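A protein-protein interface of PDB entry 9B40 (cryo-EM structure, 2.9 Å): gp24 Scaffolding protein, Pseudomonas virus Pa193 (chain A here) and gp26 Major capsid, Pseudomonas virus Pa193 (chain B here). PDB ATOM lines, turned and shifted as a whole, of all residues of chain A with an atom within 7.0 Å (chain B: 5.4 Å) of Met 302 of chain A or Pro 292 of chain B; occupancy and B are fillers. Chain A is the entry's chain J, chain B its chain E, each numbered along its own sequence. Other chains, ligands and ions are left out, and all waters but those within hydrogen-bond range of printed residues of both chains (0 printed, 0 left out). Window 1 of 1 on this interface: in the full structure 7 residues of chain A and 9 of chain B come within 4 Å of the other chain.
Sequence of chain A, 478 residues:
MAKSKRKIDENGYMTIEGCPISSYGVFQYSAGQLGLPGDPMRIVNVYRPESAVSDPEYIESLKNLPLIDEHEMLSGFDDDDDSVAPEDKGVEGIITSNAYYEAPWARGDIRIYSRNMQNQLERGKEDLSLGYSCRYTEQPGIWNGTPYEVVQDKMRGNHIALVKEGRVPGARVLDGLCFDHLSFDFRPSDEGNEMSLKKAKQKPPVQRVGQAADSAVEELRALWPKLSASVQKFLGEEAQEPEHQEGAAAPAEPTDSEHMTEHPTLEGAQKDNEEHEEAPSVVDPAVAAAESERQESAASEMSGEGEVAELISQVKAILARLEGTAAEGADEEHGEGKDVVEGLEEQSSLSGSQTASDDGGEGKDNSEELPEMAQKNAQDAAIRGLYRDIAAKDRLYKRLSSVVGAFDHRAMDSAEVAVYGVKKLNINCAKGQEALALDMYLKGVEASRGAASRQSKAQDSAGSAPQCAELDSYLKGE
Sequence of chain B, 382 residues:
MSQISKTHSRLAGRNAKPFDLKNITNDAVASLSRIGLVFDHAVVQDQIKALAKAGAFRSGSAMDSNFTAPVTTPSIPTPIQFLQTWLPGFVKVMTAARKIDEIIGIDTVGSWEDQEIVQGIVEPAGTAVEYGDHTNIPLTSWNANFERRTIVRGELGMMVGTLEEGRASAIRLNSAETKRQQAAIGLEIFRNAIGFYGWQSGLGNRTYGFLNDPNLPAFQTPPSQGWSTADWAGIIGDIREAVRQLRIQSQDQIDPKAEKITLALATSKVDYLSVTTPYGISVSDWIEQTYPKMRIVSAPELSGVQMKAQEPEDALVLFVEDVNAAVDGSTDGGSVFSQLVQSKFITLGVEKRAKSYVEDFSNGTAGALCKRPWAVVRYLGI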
ATOM      1  N   GLN A 295     -15.441 -13.657 -18.063  1.00  0.00           N
ATOM      2  CA  GLN A 295     -14.535 -13.023 -17.067  1.00  0.00           C
ATOM      3  C   GLN A 295     -15.254 -12.948 -15.717  1.00  0.00           C
ATOM      4  O   GLN A 295     -14.642 -13.331 -14.704  1.00  0.00           O
ATOM      5  CB  GLN A 295     -14.118 -11.635 -17.551  1.00  0.00           C
ATOM      6  CG  GLN A 295     -13.209 -11.665 -18.770  1.00  0.00           C
ATOM      7  CD  GLN A 295     -12.876 -10.282 -19.269  1.00  0.00           C
ATOM      8  OE1 GLN A 295     -11.713  -9.925 -19.442  1.00  0.00           O
ATOM      9  NE2 GLN A 295     -13.905  -9.484 -19.506  1.00  0.00           N
ATOM     10  N   GLU A 296     -16.503 -12.475 -15.715  1.00  0.00           N
ATOM     11  CA  GLU A 296     -17.291 -12.367 -14.458  1.00  0.00           C
ATOM     12  C   GLU A 296     -17.428 -13.752 -13.819  1.00  0.00           C
ATOM     13  O   GLU A 296     -17.009 -13.906 -12.659  1.00  0.00           O
ATOM     14  CB  GLU A 296     -18.664 -11.759 -14.748  1.00  0.00           C
ATOM     15  CG  GLU A 296     -19.180 -10.878 -13.626  1.00  0.00           C
ATOM     16  CD  GLU A 296     -18.720  -9.432 -13.696  1.00  0.00           C
ATOM     17  OE1 GLU A 296     -19.483  -8.549 -13.256  1.00  0.00           O
ATOM     18  OE2 GLU A 296     -17.602  -9.192 -14.190  1.00  0.00           O
ATOM     19  N   SER A 297     -17.997 -14.716 -14.548  1.00  0.00           N
ATOM     20  CA  SER A 297     -18.211 -16.080 -13.993  1.00  0.00           C
ATOM     21  C   SER A 297     -16.929 -16.581 -13.323  1.00  0.00           C
ATOM     22  O   SER A 297     -17.042 -17.147 -12.238  1.00  0.00           O
ATOM     23  CB  SER A 297     -18.677 -17.028 -15.067  1.00  0.00           C
ATOM     24  OG  SER A 297     -17.580 -17.505 -15.832  1.00  0.00           O
ATOM     25  N   ALA A 298     -15.767 -16.373 -13.941  1.00  0.00           N
ATOM     26  CA  ALA A 298     -14.482 -16.826 -13.420  1.00  0.00           C
ATOM     27  C   ALA A 298     -14.095 -16.059 -12.163  1.00  0.00           C
ATOM     28  O   ALA A 298     -13.815 -16.657 -11.122  1.00  0.00           O
ATOM     29  CB  ALA A 298     -13.406 -16.675 -14.495  1.00  0.00           C
ATOM     30  N   ALA A 299     -14.127 -14.724 -12.240  1.00  0.00           N
ATOM     31  CA  ALA A 299     -13.804 -13.883 -11.093  1.00  0.00           C
ATOM     32  C   ALA A 299     -14.729 -14.149  -9.912  1.00  0.00           C
ATOM     33  O   ALA A 299     -14.298 -14.077  -8.755  1.00  0.00           O
ATOM     34  CB  ALA A 299     -13.864 -12.409 -11.493  1.00  0.00           C
ATOM     35  N   SER A 300     -16.004 -14.456 -10.178  1.00  0.00           N
ATOM     36  CA  SER A 300     -16.922 -14.752  -9.082  1.00  0.00           C
ATOM     37  C   SER A 300     -16.500 -16.011  -8.341  1.00  0.00           C
ATOM     38  O   SER A 300     -16.690 -16.114  -7.125  1.00  0.00           O
ATOM     39  CB  SER A 300     -18.356 -14.897  -9.590  1.00  0.00           C
ATOM     40  OG  SER A 300     -18.450 -15.863 -10.617  1.00  0.00           O
ATOM     41  N   GLU A 301     -15.931 -16.984  -9.053  1.00  0.00           N
ATOM     42  CA  GLU A 301     -15.460 -18.188  -8.371  1.00  0.00           C
ATOM     43  C   GLU A 301     -13.969 -18.186  -8.033  1.00  0.00           C
ATOM     44  O   GLU A 301     -13.475 -19.192  -7.517  1.00  0.00           O
ATOM     45  CB  GLU A 301     -15.828 -19.436  -9.174  1.00  0.00           C
ATOM     46  CG  GLU A 301     -15.921 -19.207 -10.645  1.00  0.00           C
ATOM     47  CD  GLU A 301     -16.576 -20.350 -11.374  1.00  0.00           C
ATOM     48  OE1 GLU A 301     -17.808 -20.303 -11.567  1.00  0.00           O
ATOM     49  OE2 GLU A 301     -15.857 -21.280 -11.780  1.00  0.00           O
ATOM     50  N   MET A 302     -13.239 -17.099  -8.287  1.00  0.00           N
ATOM     51  CA  MET A 302     -11.963 -16.939  -7.599  1.00  0.00           C
ATOM     52  C   MET A 302     -12.206 -16.372  -6.207  1.00  0.00           C
ATOM     53  O   MET A 302     -13.305 -15.926  -5.877  1.00  0.00           O
ATOM     54  CB  MET A 302     -11.001 -16.017  -8.356  1.00  0.00           C
ATOM     55  CG  MET A 302     -11.083 -16.070  -9.858  1.00  0.00           C
ATOM     56  SD  MET A 302     -10.044 -14.842 -10.669  1.00  0.00           S
ATOM     57  CE  MET A 302      -9.214 -15.846 -11.896  1.00  0.00           C
ATOM     58  N   SER A 303     -11.159 -16.383  -5.386  1.00  0.00           N
ATOM     59  CA  SER A 303     -11.256 -15.857  -4.031  1.00  0.00           C
ATOM     60  C   SER A 303     -11.396 -14.332  -4.055  1.00  0.00           C
ATOM     61  O   SER A 303     -11.388 -13.692  -5.111  1.00  0.00           O
ATOM     62  CB  SER A 303     -10.049 -16.295  -3.208  1.00  0.00           C
ATOM     63  OG  SER A 303      -8.854 -15.760  -3.738  1.00  0.00           O
ATOM     64  N   GLY A 304     -11.527 -13.745  -2.865  1.00  0.00           N
ATOM     65  CA  GLY A 304     -11.867 -12.339  -2.709  1.00  0.00           C
ATOM     66  C   GLY A 304     -10.942 -11.326  -3.357  1.00  0.00           C
ATOM     67  O   GLY A 304     -11.400 -10.462  -4.112  1.00  0.00           O
ATOM     68  N   GLU A 305      -9.641 -11.411  -3.067  1.00  0.00           N
ATOM     69  CA  GLU A 305      -8.688 -10.487  -3.678  1.00  0.00           C
ATOM     70  C   GLU A 305      -8.565 -10.725  -5.175  1.00  0.00           C
ATOM     71  O   GLU A 305      -8.458  -9.772  -5.955  1.00  0.00           O
ATOM     72  CB  GLU A 305      -7.326 -10.608  -3.001  1.00  0.00           C
ATOM     73  CG  GLU A 305      -7.298  -9.983  -1.628  1.00  0.00           C
ATOM     74  CD  GLU A 305      -5.965 -10.131  -0.936  1.00  0.00           C
ATOM     75  OE1 GLU A 305      -5.642  -9.256  -0.109  1.00  0.00           O
ATOM     76  OE2 GLU A 305      -5.246 -11.114  -1.210  1.00  0.00           O
ATOM     77  N   GLY A 306      -8.577 -11.990  -5.597  1.00  0.00           N
ATOM     78  CA  GLY A 306      -8.562 -12.281  -7.019  1.00  0.00           C
ATOM     79  C   GLY A 306      -9.771 -11.717  -7.738  1.00  0.00           C
ATOM     80  O   GLY A 306      -9.654 -11.177  -8.841  1.00  0.00           O
ATOM     81  N   GLU A 307     -10.945 -11.824  -7.117  1.00  0.00           N
ATOM     82  CA  GLU A 307     -12.154 -11.243  -7.692  1.00  0.00           C
ATOM     83  C   GLU A 307     -12.061  -9.723  -7.761  1.00  0.00           C
ATOM     84  O   GLU A 307     -12.392  -9.115  -8.787  1.00  0.00           O
ATOM     85  CB  GLU A 307     -13.369 -11.671  -6.871  1.00  0.00           C
ATOM     86  CG  GLU A 307     -14.586 -10.791  -7.057  1.00  0.00           C
ATOM     87  CD  GLU A 307     -15.876 -11.577  -7.053  1.00  0.00           C
ATOM     88  OE1 GLU A 307     -16.231 -12.120  -5.987  1.00  0.00           O
ATOM     89  OE2 GLU A 307     -16.542 -11.637  -8.107  1.00  0.00           O
ATOM     90  N   GLU A 310      -9.626  -8.885 -10.609  1.00  0.00           N
ATOM     91  CA  GLU A 310     -10.113  -9.157 -11.956  1.00  0.00           C
ATOM     92  C   GLU A 310     -11.214  -8.187 -12.356  1.00  0.00           C
ATOM     93  O   GLU A 310     -11.270  -7.747 -13.511  1.00  0.00           O
ATOM     94  CB  GLU A 310     -10.615 -10.596 -12.050  1.00  0.00           C
ATOM     95  CG  GLU A 310      -9.519 -11.635 -12.218  1.00  0.00           C
ATOM     96  CD  GLU A 310      -8.660 -11.425 -13.452  1.00  0.00           C
ATOM     97  OE1 GLU A 310      -7.499 -11.876 -13.433  1.00  0.00           O
ATOM     98  OE2 GLU A 310      -9.147 -10.857 -14.453  1.00  0.00           O
ATOM     99  N   LYS B 257      -0.310 -15.825  -9.608  1.00  0.00           N
ATOM    100  CA  LYS B 257      -1.478 -15.887  -8.680  1.00  0.00           C
ATOM    101  C   LYS B 257      -2.374 -17.078  -9.032  1.00  0.00           C
ATOM    102  O   LYS B 257      -3.540 -17.073  -8.619  1.00  0.00           O
ATOM    103  CB  LYS B 257      -2.225 -14.552  -8.677  1.00  0.00           C
ATOM    104  CG  LYS B 257      -1.406 -13.361  -8.199  1.00  0.00           C
ATOM    105  CD  LYS B 257      -2.243 -12.136  -7.924  1.00  0.00           C
ATOM    106  CE  LYS B 257      -1.888 -11.466  -6.615  1.00  0.00           C
ATOM    107  NZ  LYS B 257      -0.662 -12.051  -6.023  1.00  0.00           N
ATOM    108  N   GLU B 259      -3.821 -17.910 -11.782  1.00  0.00           N
ATOM    109  CA  GLU B 259      -4.997 -17.287 -12.384  1.00  0.00           C
ATOM    110  C   GLU B 259      -5.883 -18.308 -13.086  1.00  0.00           C
ATOM    111  O   GLU B 259      -7.038 -18.520 -12.702  1.00  0.00           O
ATOM    112  CB  GLU B 259      -4.556 -16.199 -13.364  1.00  0.00           C
ATOM    113  CG  GLU B 259      -5.699 -15.442 -14.011  1.00  0.00           C
ATOM    114  CD  GLU B 259      -5.263 -14.101 -14.564  1.00  0.00           C
ATOM    115  OE1 GLU B 259      -4.103 -13.707 -14.324  1.00  0.00           O
ATOM    116  OE2 GLU B 259      -6.071 -13.453 -15.259  1.00  0.00           O
ATOM    117  N   ILE B 287      -6.038 -20.103   0.929  1.00  0.00           N
ATOM    118  CA  ILE B 287      -6.068 -20.040  -0.532  1.00  0.00           C
ATOM    119  C   ILE B 287      -6.118 -18.592  -1.003  1.00  0.00           C
ATOM    120  O   ILE B 287      -5.422 -18.206  -1.950  1.00  0.00           O
ATOM    121  CB  ILE B 287      -7.254 -20.858  -1.075  1.00  0.00           C
ATOM    122  CG1 ILE B 287      -7.065 -22.341  -0.762  1.00  0.00           C
ATOM    123  CG2 ILE B 287      -7.417 -20.653  -2.570  1.00  0.00           C
ATOM    124  CD1 ILE B 287      -8.338 -23.148  -0.847  1.00  0.00           C
ATOM    125  N   GLU B 288      -6.929 -17.765  -0.338  1.00  0.00           N
ATOM    126  CA  GLU B 288      -7.078 -16.365  -0.717  1.00  0.00           C
ATOM    127  C   GLU B 288      -5.782 -15.585  -0.546  1.00  0.00           C
ATOM    128  O   GLU B 288      -5.492 -14.683  -1.338  1.00  0.00           O
ATOM    129  CB  GLU B 288      -8.191 -15.738   0.118  1.00  0.00           C
ATOM    130  CG  GLU B 288      -8.729 -14.429  -0.399  1.00  0.00           C
ATOM    131  CD  GLU B 288      -8.338 -13.269   0.481  1.00  0.00           C
ATOM    132  OE1 GLU B 288      -7.692 -13.503   1.524  1.00  0.00           O
ATOM    133  OE2 GLU B 288      -8.704 -12.129   0.151  1.00  0.00           O
ATOM    134  N   GLN B 289      -4.998 -15.909   0.477  1.00  0.00           N
ATOM    135  CA  GLN B 289      -3.726 -15.240   0.711  1.00  0.00           C
ATOM    136  C   GLN B 289      -2.559 -15.903  -0.007  1.00  0.00           C
ATOM    137  O   GLN B 289      -1.472 -15.319  -0.056  1.00  0.00           O
ATOM    138  CB  GLN B 289      -3.433 -15.179   2.214  1.00  0.00           C
ATOM    139  CG  GLN B 289      -2.760 -16.419   2.767  1.00  0.00           C
ATOM    140  CD  GLN B 289      -2.819 -16.487   4.279  1.00  0.00           C
ATOM    141  OE1 GLN B 289      -1.793 -16.564   4.948  1.00  0.00           O
ATOM    142  NE2 GLN B 289      -4.027 -16.451   4.825  1.00  0.00           N
ATOM    143  N   THR B 290      -2.755 -17.092  -0.571  1.00  0.00           N
ATOM    144  CA  THR B 290      -1.697 -17.820  -1.259  1.00  0.00           C
ATOM    145  C   THR B 290      -1.904 -17.888  -2.763  1.00  0.00           C
ATOM    146  O   THR B 290      -1.000 -17.543  -3.529  1.00  0.00           O
ATOM    147  CB  THR B 290      -1.589 -19.240  -0.693  1.00  0.00           C
ATOM    148  OG1 THR B 290      -1.253 -19.180   0.698  1.00  0.00           O
ATOM    149  CG2 THR B 290      -0.528 -20.003  -1.426  1.00  0.00           C
ATOM    150  N   TYR B 291      -3.085 -18.305  -3.209  1.00  0.00           N
ATOM    151  CA  TYR B 291      -3.422 -18.378  -4.630  1.00  0.00           C
ATOM    152  C   TYR B 291      -4.698 -17.577  -4.846  1.00  0.00           C
ATOM    153  O   TYR B 291      -5.788 -18.145  -4.981  1.00  0.00           O
ATOM    154  CB  TYR B 291      -3.596 -19.827  -5.082  1.00  0.00           C
ATOM    155  CG  TYR B 291      -2.449 -20.737  -4.705  1.00  0.00           C
ATOM    156  CD1 TYR B 291      -1.170 -20.514  -5.194  1.00  0.00           C
ATOM    157  CD2 TYR B 291      -2.651 -21.826  -3.870  1.00  0.00           C
ATOM    158  CE1 TYR B 291      -0.120 -21.345  -4.852  1.00  0.00           C
ATOM    159  CE2 TYR B 291      -1.611 -22.665  -3.525  1.00  0.00           C
ATOM    160  CZ  TYR B 291      -0.348 -22.418  -4.017  1.00  0.00           C
ATOM    161  OH  TYR B 291       0.691 -23.250  -3.675  1.00  0.00           O
ATOM    162  N   PRO B 292      -4.598 -16.240  -4.845  1.00  0.00           N
ATOM    163  CA  PRO B 292      -5.814 -15.409  -4.832  1.00  0.00           C
ATOM    164  C   PRO B 292      -6.715 -15.592  -6.038  1.00  0.00           C
ATOM    165  O   PRO B 292      -7.942 -15.508  -5.902  1.00  0.00           O
ATOM    166  CB  PRO B 292      -5.255 -13.983  -4.763  1.00  0.00           C
ATOM    167  CG  PRO B 292      -3.894 -14.126  -4.199  1.00  0.00           C
ATOM    168  CD  PRO B 292      -3.376 -15.431  -4.707  1.00  0.00           C
ATOM    169  N   LYS B 293      -6.149 -15.835  -7.219  1.00  0.00           N
ATOM    170  CA  LYS B 293      -6.934 -15.970  -8.438  1.00  0.00           C
ATOM    171  C   LYS B 293      -7.173 -17.426  -8.815  1.00  0.00           C
ATOM    172  O   LYS B 293      -7.361 -17.739  -9.993  1.00  0.00           O
ATOM    173  CB  LYS B 293      -6.260 -15.222  -9.586  1.00  0.00           C
ATOM    174  CG  LYS B 293      -6.322 -13.715  -9.437  1.00  0.00           C
ATOM    175  CD  LYS B 293      -5.140 -13.032 -10.080  1.00  0.00           C
ATOM    176  CE  LYS B 293      -5.396 -11.550 -10.253  1.00  0.00           C
ATOM    177  NZ  LYS B 293      -6.076 -11.257 -11.539  1.00  0.00           N
ATOM    178  N   MET B 294      -7.192 -18.321  -7.835  1.00  0.00           N
ATOM    179  CA  MET B 294      -7.473 -19.730  -8.080  1.00  0.00           C
ATOM    180  C   MET B 294      -8.983 -19.921  -8.100  1.00  0.00           C
ATOM    181  O   MET B 294      -9.657 -19.698  -7.091  1.00  0.00           O
ATOM    182  CB  MET B 294      -6.826 -20.612  -7.018  1.00  0.00           C
ATOM    183  CG  MET B 294      -7.067 -22.094  -7.234  1.00  0.00           C
ATOM    184  SD  MET B 294      -6.791 -23.070  -5.748  1.00  0.00           S
ATOM    185  CE  MET B 294      -5.077 -23.524  -5.966  1.00  0.00           C
ATOM    186  N   ARG B 295      -9.512 -20.307  -9.256  1.00  0.00           N
ATOM    187  CA  ARG B 295     -10.919 -20.663  -9.360  1.00  0.00           C
ATOM    188  C   ARG B 295     -11.206 -21.904  -8.529  1.00  0.00           C
ATOM    189  O   ARG B 295     -10.440 -22.867  -8.558  1.00  0.00           O
ATOM    190  CB  ARG B 295     -11.273 -20.901 -10.825  1.00  0.00           C
ATOM    191  CG  ARG B 295     -12.700 -20.609 -11.193  1.00  0.00           C
ATOM    192  CD  ARG B 295     -12.824 -20.424 -12.691  1.00  0.00           C
ATOM    193  NE  ARG B 295     -12.844 -21.697 -13.402  1.00  0.00           N
ATOM    194  CZ  ARG B 295     -13.915 -22.218 -13.983  1.00  0.00           C
ATOM    195  NH1 ARG B 295     -15.079 -21.592 -13.975  1.00  0.00           N
ATOM    196  NH2 ARG B 295     -13.812 -23.395 -14.594  1.00  0.00           N
ATOM    197  N   ILE B 296     -12.302 -21.878  -7.775  1.00  0.00           N
ATOM    198  CA  ILE B 296     -12.695 -22.994  -6.922  1.00  0.00           C
ATOM    199  C   ILE B 296     -14.127 -23.372  -7.265  1.00  0.00           C
ATOM    200  O   ILE B 296     -15.020 -22.519  -7.227  1.00  0.00           O
ATOM    201  CB  ILE B 296     -12.583 -22.643  -5.426  1.00  0.00           C
ATOM    202  CG1 ILE B 296     -11.132 -22.369  -5.037  1.00  0.00           C
ATOM    203  CG2 ILE B 296     -13.144 -23.765  -4.572  1.00  0.00           C
ATOM    204  CD1 ILE B 296     -10.919 -21.012  -4.416  1.00  0.00           C
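Of the 14 printed residues of chain A, 7 touch a printed residue of chain B. Hydrophobic or aromatic side chains of chain A that line the printed part of chain B: Met 302. Along chain B the printed residues that touch a printed residue of chain A span positions 259 to 296.
Among the printed residues, merely in contact across the chains: Met 302 of chain A with Lys 293 of chain B (3.3 Å), Gly 306 of chain A with Pro 292 of chain B (3.5 Å), Met 302 of chain A with Glu 259 of chain B (3.5 Å), Ser 303 of chain A with Glu 288 of chain B (3.6 Å), Gly 306 of chain A with Lys 293 of chain B (3.6 Å), Met 302 of chain A with Met 294 of chain B (3.6 Å), Gly 304 of chain A with Glu 288 of chain B (3.8 Å), Glu 301 of chain A with Met 294 of chain B (3.9 Å) and Met 302 of chain A with Pro 292 of chain B (3.95 Å).
Of the printed residues of chain A, Pro 292 of chain B touches Met 302 (3.95 Å), Ser 303 (2.4 Å) and Gly 306 (3.5 Å). Of the printed residues of chain A, Lys 293 of chain B touches Met 302, Gly 306 and Glu 310. Printed residues of chain B within 4 Å of Ser 303 of chain A: Glu 288 (3.6 Å) and Pro 292 (2.4 Å). Of the printed residues of chain B, Glu 310 of chain A touches Glu 259 (2.8 Å) and Lys 293 (2.4 Å). The nearest residue of chain B that does not touch Met 302 of chain A is Arg 295 of chain B (4.2 Å). The nearest residue of chain A that does not touch Pro 292 of chain B is Glu 305 of chain A (4.3 Å).
The backbone NH of Lys 293 of chain B is in hydrogen-bond range of the backbone carbonyl oxygen of Lys 257 of chain B, at 3.2 Å.
The backbone carbonyl oxygen (O) of Glu 301 of chain A lies within hydrogen-bond range of the backbone NH (N) of Ile 296 of chain B (2.9 Å). The backbone carbonyl oxygen (O) of Pro 292 of chain B lies within hydrogen-bond range of the backbone NH (N) of Ser 303 of chain A, at 3.4 Å. NZ of Lys 293 of chain B lies within salt-bridge range of OE1 of Glu 310 of chain A (2.4 Å). OE2 of Glu 259 of chain B lies close to OE1 of Glu 310 of chain A. OE2 of Glu 301 of chain A lies within salt-bridge range of NE of Arg 295 of chain B (3.4 Å). OE2 of Glu 288 of chain B lies close to N of Glu 305 of chain A (3.4 Å).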
